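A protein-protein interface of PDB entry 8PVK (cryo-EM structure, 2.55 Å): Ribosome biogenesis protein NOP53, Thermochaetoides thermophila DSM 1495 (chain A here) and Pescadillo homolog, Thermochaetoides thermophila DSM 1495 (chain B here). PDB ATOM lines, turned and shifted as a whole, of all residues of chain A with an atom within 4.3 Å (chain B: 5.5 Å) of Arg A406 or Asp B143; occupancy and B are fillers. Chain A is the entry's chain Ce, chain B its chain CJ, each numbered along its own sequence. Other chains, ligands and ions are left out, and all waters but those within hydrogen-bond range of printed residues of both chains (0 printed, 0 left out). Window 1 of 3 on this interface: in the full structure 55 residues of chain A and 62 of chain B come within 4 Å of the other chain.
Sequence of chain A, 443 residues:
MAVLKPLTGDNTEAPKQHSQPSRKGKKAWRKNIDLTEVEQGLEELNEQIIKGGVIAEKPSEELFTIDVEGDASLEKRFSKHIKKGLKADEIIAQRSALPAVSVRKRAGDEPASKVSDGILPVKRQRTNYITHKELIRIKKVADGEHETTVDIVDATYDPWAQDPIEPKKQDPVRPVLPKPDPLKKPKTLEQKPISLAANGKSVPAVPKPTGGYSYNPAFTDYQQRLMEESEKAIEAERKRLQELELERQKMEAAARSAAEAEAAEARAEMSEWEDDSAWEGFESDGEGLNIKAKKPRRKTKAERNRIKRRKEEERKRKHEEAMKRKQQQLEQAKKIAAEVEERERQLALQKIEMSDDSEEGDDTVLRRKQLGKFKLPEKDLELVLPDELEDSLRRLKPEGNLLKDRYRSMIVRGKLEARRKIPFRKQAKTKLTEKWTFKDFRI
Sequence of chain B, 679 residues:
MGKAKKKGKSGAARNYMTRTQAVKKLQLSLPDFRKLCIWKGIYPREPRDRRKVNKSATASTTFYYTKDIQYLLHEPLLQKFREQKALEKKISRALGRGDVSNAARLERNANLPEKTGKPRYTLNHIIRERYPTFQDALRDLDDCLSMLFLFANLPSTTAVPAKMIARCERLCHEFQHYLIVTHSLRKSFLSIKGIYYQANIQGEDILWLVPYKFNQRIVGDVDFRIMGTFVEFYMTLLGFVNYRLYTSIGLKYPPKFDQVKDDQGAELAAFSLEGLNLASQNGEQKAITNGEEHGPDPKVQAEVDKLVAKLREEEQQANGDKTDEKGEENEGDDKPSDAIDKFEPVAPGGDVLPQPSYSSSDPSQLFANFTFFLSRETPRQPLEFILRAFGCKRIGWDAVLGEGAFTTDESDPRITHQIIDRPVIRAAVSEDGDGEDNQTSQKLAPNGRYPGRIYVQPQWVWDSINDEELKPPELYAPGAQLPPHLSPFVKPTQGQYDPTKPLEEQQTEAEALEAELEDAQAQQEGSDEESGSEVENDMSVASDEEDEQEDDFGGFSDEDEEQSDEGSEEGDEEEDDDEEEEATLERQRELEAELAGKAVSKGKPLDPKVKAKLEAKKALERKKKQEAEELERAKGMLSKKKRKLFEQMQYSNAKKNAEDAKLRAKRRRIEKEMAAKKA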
ATOM      1  N   ALA A 205      12.330   7.056  17.267  1.00  0.00           N
ATOM      2  CA  ALA A 205      11.752   8.273  16.704  1.00  0.00           C
ATOM      3  C   ALA A 205      10.683   8.849  17.623  1.00  0.00           C
ATOM      4  O   ALA A 205      10.683  10.050  17.917  1.00  0.00           O
ATOM      5  CB  ALA A 205      11.177   7.986  15.317  1.00  0.00           C
ATOM      6  N   LEU A 402       6.145  20.574  19.783  1.00  0.00           N
ATOM      7  CA  LEU A 402       6.339  19.338  19.035  1.00  0.00           C
ATOM      8  C   LEU A 402       7.259  19.536  17.836  1.00  0.00           C
ATOM      9  O   LEU A 402       7.980  18.607  17.458  1.00  0.00           O
ATOM     10  CB  LEU A 402       4.991  18.769  18.595  1.00  0.00           C
ATOM     11  CG  LEU A 402       4.105  18.206  19.711  1.00  0.00           C
ATOM     12  CD1 LEU A 402       3.043  17.292  19.135  1.00  0.00           C
ATOM     13  CD2 LEU A 402       4.920  17.472  20.768  1.00  0.00           C
ATOM     14  N   LEU A 403       7.255  20.727  17.234  1.00  0.00           N
ATOM     15  CA  LEU A 403       8.202  21.014  16.158  1.00  0.00           C
ATOM     16  C   LEU A 403       9.636  21.006  16.673  1.00  0.00           C
ATOM     17  O   LEU A 403      10.533  20.436  16.035  1.00  0.00           O
ATOM     18  CB  LEU A 403       7.862  22.357  15.515  1.00  0.00           C
ATOM     19  CG  LEU A 403       8.632  22.745  14.255  1.00  0.00           C
ATOM     20  CD1 LEU A 403       8.507  21.658  13.202  1.00  0.00           C
ATOM     21  CD2 LEU A 403       8.126  24.072  13.719  1.00  0.00           C
ATOM     22  N   LYS A 404       9.859  21.614  17.840  1.00  0.00           N
ATOM     23  CA  LYS A 404      11.166  21.563  18.480  1.00  0.00           C
ATOM     24  C   LYS A 404      11.533  20.142  18.881  1.00  0.00           C
ATOM     25  O   LYS A 404      12.705  19.762  18.798  1.00  0.00           O
ATOM     26  CB  LYS A 404      11.183  22.486  19.697  1.00  0.00           C
ATOM     27  CG  LYS A 404      12.566  22.941  20.122  1.00  0.00           C
ATOM     28  CD  LYS A 404      12.477  24.036  21.170  1.00  0.00           C
ATOM     29  CE  LYS A 404      13.846  24.606  21.496  1.00  0.00           C
ATOM     30  NZ  LYS A 404      13.768  25.665  22.538  1.00  0.00           N
ATOM     31  N   ASP A 405      10.544  19.347  19.302  1.00  0.00           N
ATOM     32  CA  ASP A 405      10.796  17.952  19.646  1.00  0.00           C
ATOM     33  C   ASP A 405      11.235  17.149  18.429  1.00  0.00           C
ATOM     34  O   ASP A 405      12.159  16.334  18.520  1.00  0.00           O
ATOM     35  CB  ASP A 405       9.546  17.335  20.271  1.00  0.00           C
ATOM     36  CG  ASP A 405       9.520  17.476  21.778  1.00  0.00           C
ATOM     37  OD1 ASP A 405      10.482  18.040  22.341  1.00  0.00           O
ATOM     38  OD2 ASP A 405       8.537  17.023  22.401  1.00  0.00           O
ATOM     39  N   ARG A 406      10.590  17.366  17.280  1.00  0.00           N
ATOM     40  CA  ARG A 406      10.974  16.647  16.067  1.00  0.00           C
ATOM     41  C   ARG A 406      12.347  17.084  15.570  1.00  0.00           C
ATOM     42  O   ARG A 406      13.139  16.250  15.110  1.00  0.00           O
ATOM     43  CB  ARG A 406       9.921  16.839  14.976  1.00  0.00           C
ATOM     44  CG  ARG A 406       8.552  16.264  15.309  1.00  0.00           C
ATOM     45  CD  ARG A 406       8.311  14.910  14.649  1.00  0.00           C
ATOM     46  NE  ARG A 406       9.323  13.920  14.996  1.00  0.00           N
ATOM     47  CZ  ARG A 406       9.351  13.236  16.132  1.00  0.00           C
ATOM     48  NH1 ARG A 406       8.427  13.405  17.064  1.00  0.00           N
ATOM     49  NH2 ARG A 406      10.328  12.359  16.338  1.00  0.00           N
ATOM     50  N   TYR A 407      12.648  18.384  15.658  1.00  0.00           N
ATOM     51  CA  TYR A 407      13.975  18.866  15.277  1.00  0.00           C
ATOM     52  C   TYR A 407      15.059  18.287  16.185  1.00  0.00           C
ATOM     53  O   TYR A 407      16.115  17.843  15.705  1.00  0.00           O
ATOM     54  CB  TYR A 407      13.990  20.395  15.309  1.00  0.00           C
ATOM     55  CG  TYR A 407      15.249  21.030  14.769  1.00  0.00           C
ATOM     56  CD1 TYR A 407      15.688  20.762  13.479  1.00  0.00           C
ATOM     57  CD2 TYR A 407      15.985  21.918  15.541  1.00  0.00           C
ATOM     58  CE1 TYR A 407      16.834  21.347  12.979  1.00  0.00           C
ATOM     59  CE2 TYR A 407      17.130  22.512  15.049  1.00  0.00           C
ATOM     60  CZ  TYR A 407      17.552  22.221  13.769  1.00  0.00           C
ATOM     61  OH  TYR A 407      18.694  22.808  13.277  1.00  0.00           O
ATOM     62  N   ARG A 408      14.799  18.255  17.497  1.00  0.00           N
ATOM     63  CA  ARG A 408      15.739  17.654  18.436  1.00  0.00           C
ATOM     64  C   ARG A 408      15.893  16.160  18.193  1.00  0.00           C
ATOM     65  O   ARG A 408      16.988  15.614  18.348  1.00  0.00           O
ATOM     66  CB  ARG A 408      15.283  17.909  19.872  1.00  0.00           C
ATOM     67  CG  ARG A 408      15.744  19.229  20.453  1.00  0.00           C
ATOM     68  CD  ARG A 408      15.481  19.267  21.944  1.00  0.00           C
ATOM     69  NE  ARG A 408      16.055  18.105  22.614  1.00  0.00           N
ATOM     70  CZ  ARG A 408      17.110  18.148  23.416  1.00  0.00           C
ATOM     71  NH1 ARG A 408      17.729  19.286  23.683  1.00  0.00           N
ATOM     72  NH2 ARG A 408      17.552  17.020  23.965  1.00  0.00           N
ATOM     73  N   SER A 409      14.803  15.482  17.826  1.00  0.00           N
ATOM     74  CA  SER A 409      14.878  14.058  17.515  1.00  0.00           C
ATOM     75  C   SER A 409      15.739  13.809  16.286  1.00  0.00           C
ATOM     76  O   SER A 409      16.531  12.859  16.261  1.00  0.00           O
ATOM     77  CB  SER A 409      13.473  13.493  17.312  1.00  0.00           C
ATOM     78  OG  SER A 409      13.522  12.118  16.976  1.00  0.00           O
ATOM     79  N   MET A 410      15.604  14.661  15.264  1.00  0.00           N
ATOM     80  CA  MET A 410      16.449  14.553  14.075  1.00  0.00           C
ATOM     81  C   MET A 410      17.922  14.737  14.427  1.00  0.00           C
ATOM     82  O   MET A 410      18.781  13.962  13.985  1.00  0.00           O
ATOM     83  CB  MET A 410      16.026  15.589  13.034  1.00  0.00           C
ATOM     84  CG  MET A 410      14.704  15.317  12.342  1.00  0.00           C
ATOM     85  SD  MET A 410      14.358  13.576  12.056  1.00  0.00           S
ATOM     86  CE  MET A 410      12.742  13.697  11.293  1.00  0.00           C
ATOM     87  N   ARG A 413      19.151  11.670  16.687  1.00  0.00           N
ATOM     88  CA  ARG A 413      19.321  10.462  15.891  1.00  0.00           C
ATOM     89  C   ARG A 413      20.350  10.627  14.782  1.00  0.00           C
ATOM     90  O   ARG A 413      20.747   9.623  14.181  1.00  0.00           O
ATOM     91  CB  ARG A 413      17.977  10.031  15.308  1.00  0.00           C
ATOM     92  CG  ARG A 413      17.056   9.390  16.331  1.00  0.00           C
ATOM     93  CD  ARG A 413      15.771   8.916  15.690  1.00  0.00           C
ATOM     94  NE  ARG A 413      14.923  10.035  15.305  1.00  0.00           N
ATOM     95  CZ  ARG A 413      14.207  10.081  14.192  1.00  0.00           C
ATOM     96  NH1 ARG A 413      14.208   9.080  13.327  1.00  0.00           N
ATOM     97  NH2 ARG A 413      13.469  11.159  13.940  1.00  0.00           N
ATOM     98  N   ARG B 139       8.108   0.664   9.296  1.00  0.00           N
ATOM     99  CA  ARG B 139       8.915   1.002  10.462  1.00  0.00           C
ATOM    100  C   ARG B 139       9.260   2.487  10.520  1.00  0.00           C
ATOM    101  O   ARG B 139       9.425   3.031  11.616  1.00  0.00           O
ATOM    102  CB  ARG B 139      10.187   0.154  10.480  1.00  0.00           C
ATOM    103  CG  ARG B 139       9.936  -1.302  10.843  1.00  0.00           C
ATOM    104  CD  ARG B 139      11.220  -2.026  11.207  1.00  0.00           C
ATOM    105  NE  ARG B 139      12.005  -2.377  10.029  1.00  0.00           N
ATOM    106  CZ  ARG B 139      11.958  -3.557   9.426  1.00  0.00           C
ATOM    107  NH1 ARG B 139      11.169  -4.524   9.862  1.00  0.00           N
ATOM    108  NH2 ARG B 139      12.723  -3.770   8.360  1.00  0.00           N
ATOM    109  N   ASP B 140       9.376   3.156   9.373  1.00  0.00           N
ATOM    110  CA  ASP B 140       9.618   4.598   9.371  1.00  0.00           C
ATOM    111  C   ASP B 140       8.324   5.416   9.414  1.00  0.00           C
ATOM    112  O   ASP B 140       8.372   6.658   9.522  1.00  0.00           O
ATOM    113  CB  ASP B 140      10.455   4.985   8.147  1.00  0.00           C
ATOM    114  CG  ASP B 140      11.140   6.327   8.308  1.00  0.00           C
ATOM    115  OD1 ASP B 140      12.117   6.408   9.081  1.00  0.00           O
ATOM    116  OD2 ASP B 140      10.704   7.299   7.658  1.00  0.00           O
ATOM    117  N   LEU B 141       7.168   4.745   9.340  1.00  0.00           N
ATOM    118  CA  LEU B 141       5.892   5.443   9.462  1.00  0.00           C
ATOM    119  C   LEU B 141       5.706   6.162  10.793  1.00  0.00           C
ATOM    120  O   LEU B 141       4.883   7.074  10.851  1.00  0.00           O
ATOM    121  CB  LEU B 141       4.712   4.491   9.263  1.00  0.00           C
ATOM    122  CG  LEU B 141       4.340   4.116   7.833  1.00  0.00           C
ATOM    123  CD1 LEU B 141       3.103   3.247   7.845  1.00  0.00           C
ATOM    124  CD2 LEU B 141       4.121   5.359   6.992  1.00  0.00           C
ATOM    125  N   ASP B 142       6.433   5.791  11.851  1.00  0.00           N
ATOM    126  CA  ASP B 142       6.339   6.534  13.110  1.00  0.00           C
ATOM    127  C   ASP B 142       6.754   7.988  12.922  1.00  0.00           C
ATOM    128  O   ASP B 142       5.980   8.917  13.206  1.00  0.00           O
ATOM    129  CB  ASP B 142       7.218   5.875  14.174  1.00  0.00           C
ATOM    130  CG  ASP B 142       6.696   4.530  14.610  1.00  0.00           C
ATOM    131  OD1 ASP B 142       5.470   4.331  14.560  1.00  0.00           O
ATOM    132  OD2 ASP B 142       7.513   3.671  15.005  1.00  0.00           O
ATOM    133  N   ASP B 143       7.965   8.195  12.397  1.00  0.00           N
ATOM    134  CA  ASP B 143       8.458   9.539  12.127  1.00  0.00           C
ATOM    135  C   ASP B 143       7.625  10.225  11.055  1.00  0.00           C
ATOM    136  O   ASP B 143       7.318  11.421  11.172  1.00  0.00           O
ATOM    137  CB  ASP B 143       9.925   9.472  11.706  1.00  0.00           C
ATOM    138  CG  ASP B 143      10.731  10.642  12.217  1.00  0.00           C
ATOM    139  OD1 ASP B 143      10.129  11.601  12.745  1.00  0.00           O
ATOM    140  OD2 ASP B 143      11.971  10.599  12.091  1.00  0.00           O
ATOM    141  N   CYS B 144       7.236   9.476  10.012  1.00  0.00           N
ATOM    142  CA  CYS B 144       6.439  10.059   8.933  1.00  0.00           C
ATOM    143  C   CYS B 144       5.098  10.586   9.443  1.00  0.00           C
ATOM    144  O   CYS B 144       4.709  11.724   9.148  1.00  0.00           O
ATOM    145  CB  CYS B 144       6.223   9.025   7.830  1.00  0.00           C
ATOM    146  SG  CYS B 144       5.112   9.560   6.512  1.00  0.00           S
ATOM    147  N   LEU B 145       4.399   9.781  10.248  1.00  0.00           N
ATOM    148  CA  LEU B 145       3.082  10.158  10.741  1.00  0.00           C
ATOM    149  C   LEU B 145       3.169  11.280  11.760  1.00  0.00           C
ATOM    150  O   LEU B 145       2.313  12.171  11.769  1.00  0.00           O
ATOM    151  CB  LEU B 145       2.387   8.944  11.349  1.00  0.00           C
ATOM    152  CG  LEU B 145       1.783   7.959  10.356  1.00  0.00           C
ATOM    153  CD1 LEU B 145       1.478   6.663  11.069  1.00  0.00           C
ATOM    154  CD2 LEU B 145       0.537   8.543   9.722  1.00  0.00           C
ATOM    155  N   SER B 146       4.188  11.255  12.630  1.00  0.00           N
ATOM    156  CA  SER B 146       4.348  12.349  13.583  1.00  0.00           C
ATOM    157  C   SER B 146       4.596  13.671  12.867  1.00  0.00           C
ATOM    158  O   SER B 146       3.941  14.679  13.168  1.00  0.00           O
ATOM    159  CB  SER B 146       5.486  12.040  14.553  1.00  0.00           C
ATOM    160  OG  SER B 146       5.130  10.982  15.425  1.00  0.00           O
ATOM    161  N   MET B 147       5.487  13.665  11.867  1.00  0.00           N
ATOM    162  CA  MET B 147       5.793  14.885  11.125  1.00  0.00           C
ATOM    163  C   MET B 147       4.576  15.397  10.360  1.00  0.00           C
ATOM    164  O   MET B 147       4.274  16.597  10.380  1.00  0.00           O
ATOM    165  CB  MET B 147       6.961  14.625  10.175  1.00  0.00           C
ATOM    166  CG  MET B 147       7.494  15.861   9.483  1.00  0.00           C
ATOM    167  SD  MET B 147       8.271  17.017  10.624  1.00  0.00           S
ATOM    168  CE  MET B 147       9.775  16.131  11.018  1.00  0.00           C
ATOM    169  N   LEU B 148       3.839  14.495   9.703  1.00  0.00           N
ATOM    170  CA  LEU B 148       2.717  14.943   8.886  1.00  0.00           C
ATOM    171  C   LEU B 148       1.515  15.372   9.720  1.00  0.00           C
ATOM    172  O   LEU B 148       0.856  16.361   9.375  1.00  0.00           O
ATOM    173  CB  LEU B 148       2.327  13.853   7.888  1.00  0.00           C
ATOM    174  CG  LEU B 148       3.345  13.651   6.760  1.00  0.00           C
ATOM    175  CD1 LEU B 148       2.762  12.811   5.647  1.00  0.00           C
ATOM    176  CD2 LEU B 148       3.844  14.981   6.209  1.00  0.00           C
ATOM    177  N   LEU B 150       1.789  16.660  12.636  1.00  0.00           N
ATOM    178  CA  LEU B 150       2.189  17.950  13.183  1.00  0.00           C
ATOM    179  C   LEU B 150       2.008  19.064  12.158  1.00  0.00           C
ATOM    180  O   LEU B 150       1.482  20.136  12.479  1.00  0.00           O
ATOM    181  CB  LEU B 150       3.638  17.881  13.657  1.00  0.00           C
ATOM    182  CG  LEU B 150       4.306  19.180  14.096  1.00  0.00           C
ATOM    183  CD1 LEU B 150       3.541  19.842  15.232  1.00  0.00           C
ATOM    184  CD2 LEU B 150       5.731  18.882  14.500  1.00  0.00           C
ATOM    185  N   MET B 227      12.936  21.285   7.836  1.00  0.00           N
ATOM    186  CA  MET B 227      11.759  20.555   8.292  1.00  0.00           C
ATOM    187  C   MET B 227      10.746  20.394   7.165  1.00  0.00           C
ATOM    188  O   MET B 227      10.136  19.332   7.017  1.00  0.00           O
ATOM    189  CB  MET B 227      11.127  21.269   9.486  1.00  0.00           C
ATOM    190  CG  MET B 227      11.833  21.017  10.807  1.00  0.00           C
ATOM    191  SD  MET B 227      11.590  19.340  11.418  1.00  0.00           S
ATOM    192  CE  MET B 227      13.283  18.766  11.509  1.00  0.00           C
ATOM    193  N   TYR B 234       8.236  12.951   3.452  1.00  0.00           N
ATOM    194  CA  TYR B 234       7.304  12.097   4.174  1.00  0.00           C
ATOM    195  C   TYR B 234       5.937  12.036   3.502  1.00  0.00           C
ATOM    196  O   TYR B 234       5.278  10.994   3.567  1.00  0.00           O
ATOM    197  CB  TYR B 234       7.187  12.561   5.623  1.00  0.00           C
ATOM    198  CG  TYR B 234       8.332  12.066   6.475  1.00  0.00           C
ATOM    199  CD1 TYR B 234       8.919  10.833   6.225  1.00  0.00           C
ATOM    200  CD2 TYR B 234       8.833  12.830   7.520  1.00  0.00           C
ATOM    201  CE1 TYR B 234       9.968  10.372   6.990  1.00  0.00           C
ATOM    202  CE2 TYR B 234       9.884  12.374   8.295  1.00  0.00           C
ATOM    203  CZ  TYR B 234      10.446  11.144   8.024  1.00  0.00           C
ATOM    204  OH  TYR B 234      11.491  10.684   8.790  1.00  0.00           O
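Of chain B, only Asp B143 and Leu B150 come within 4 Å of Arg A406. Asp B143 touches just these residues of chain A: Arg A406 (3.3 Å), Met A410 (3.3 Å) and Arg A413 (2.4 Å). Of the printed residues of chain B, Leu A402 touches Leu B150 (3.7 Å). Printed residues of chain B within 4 Å of Tyr A407: Met B227. Printed residues of chain A within 4 Å of Leu B150: Leu A402, Leu A403 and Arg A406. Of the printed residues of chain A, Met B227 touches Tyr A407 and Met A410. Leu B145 touches none of the printed residues of chain A. Ala A205 touches none of the printed residues of chain B. The nearest printed residue of chain B that does not touch Arg A406 is Met B147 (4.02 Å). The nearest printed residue of chain A that does not touch Leu B150 is Lys A404 (6.0 Å).
Among the printed residues, merely in contact across the chains: Met A410 with Asp B143 (3.3 Å), Leu A403 with Leu B150 (3.6 Å), Tyr A407 with Met B227 (3.7 Å), Leu A402 with Leu B150 (3.7 Å), Met A410 with Met B227 (3.8 Å), Met A410 with Met B147 (3.8 Å) and Arg A406 with Leu B150 (3.9 Å).
NH2 of Arg A406 is in hydrogen-bond range of O of Ala A205 (2.8 Å). The side-chain hydroxyl of Ser A409 sits at hydrogen-bond distance from the guanidinium group of Arg A406 (3.3 Å). The guanidinium group (NE) of Arg A413 sits at hydrogen-bond distance from the side-chain hydroxyl (OG) of Ser A409, 3.0 Å away. NH2 of Arg A413 lies within hydrogen-bond range of SD of Met A410, at 3.2 Å. The side-chain carboxylate of Asp B143 lies within hydrogen-bond range of the side-chain hydroxyl of Tyr B234 (3.3 Å).
Of the 13 printed residues of chain B, 4 touch a printed residue of chain A. Printed residues of chain B that touch a printed residue of chain A: Asp B143, Met B147, Leu B150 and Met B227. Of the 11 printed residues of chain A, 6 touch a printed residue of chain B. Printed residues of chain A that touch a printed residue of chain B: Leu A402, Leu A403, Arg A406, Tyr A407, Met A410 and Arg A413. Among the printed residues, Asp or Glu carboxylates within 4 Å of a Lys or Arg side-chain nitrogen of the other chain: Arg A406 with Asp B143 and Arg A413 with Asp B143.
OD1 of Asp B143 is in salt-bridge range of NE of Arg A406. OD2 of Asp B143 lies within salt-bridge range of NH2 of Arg A413 (2.4 Å).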
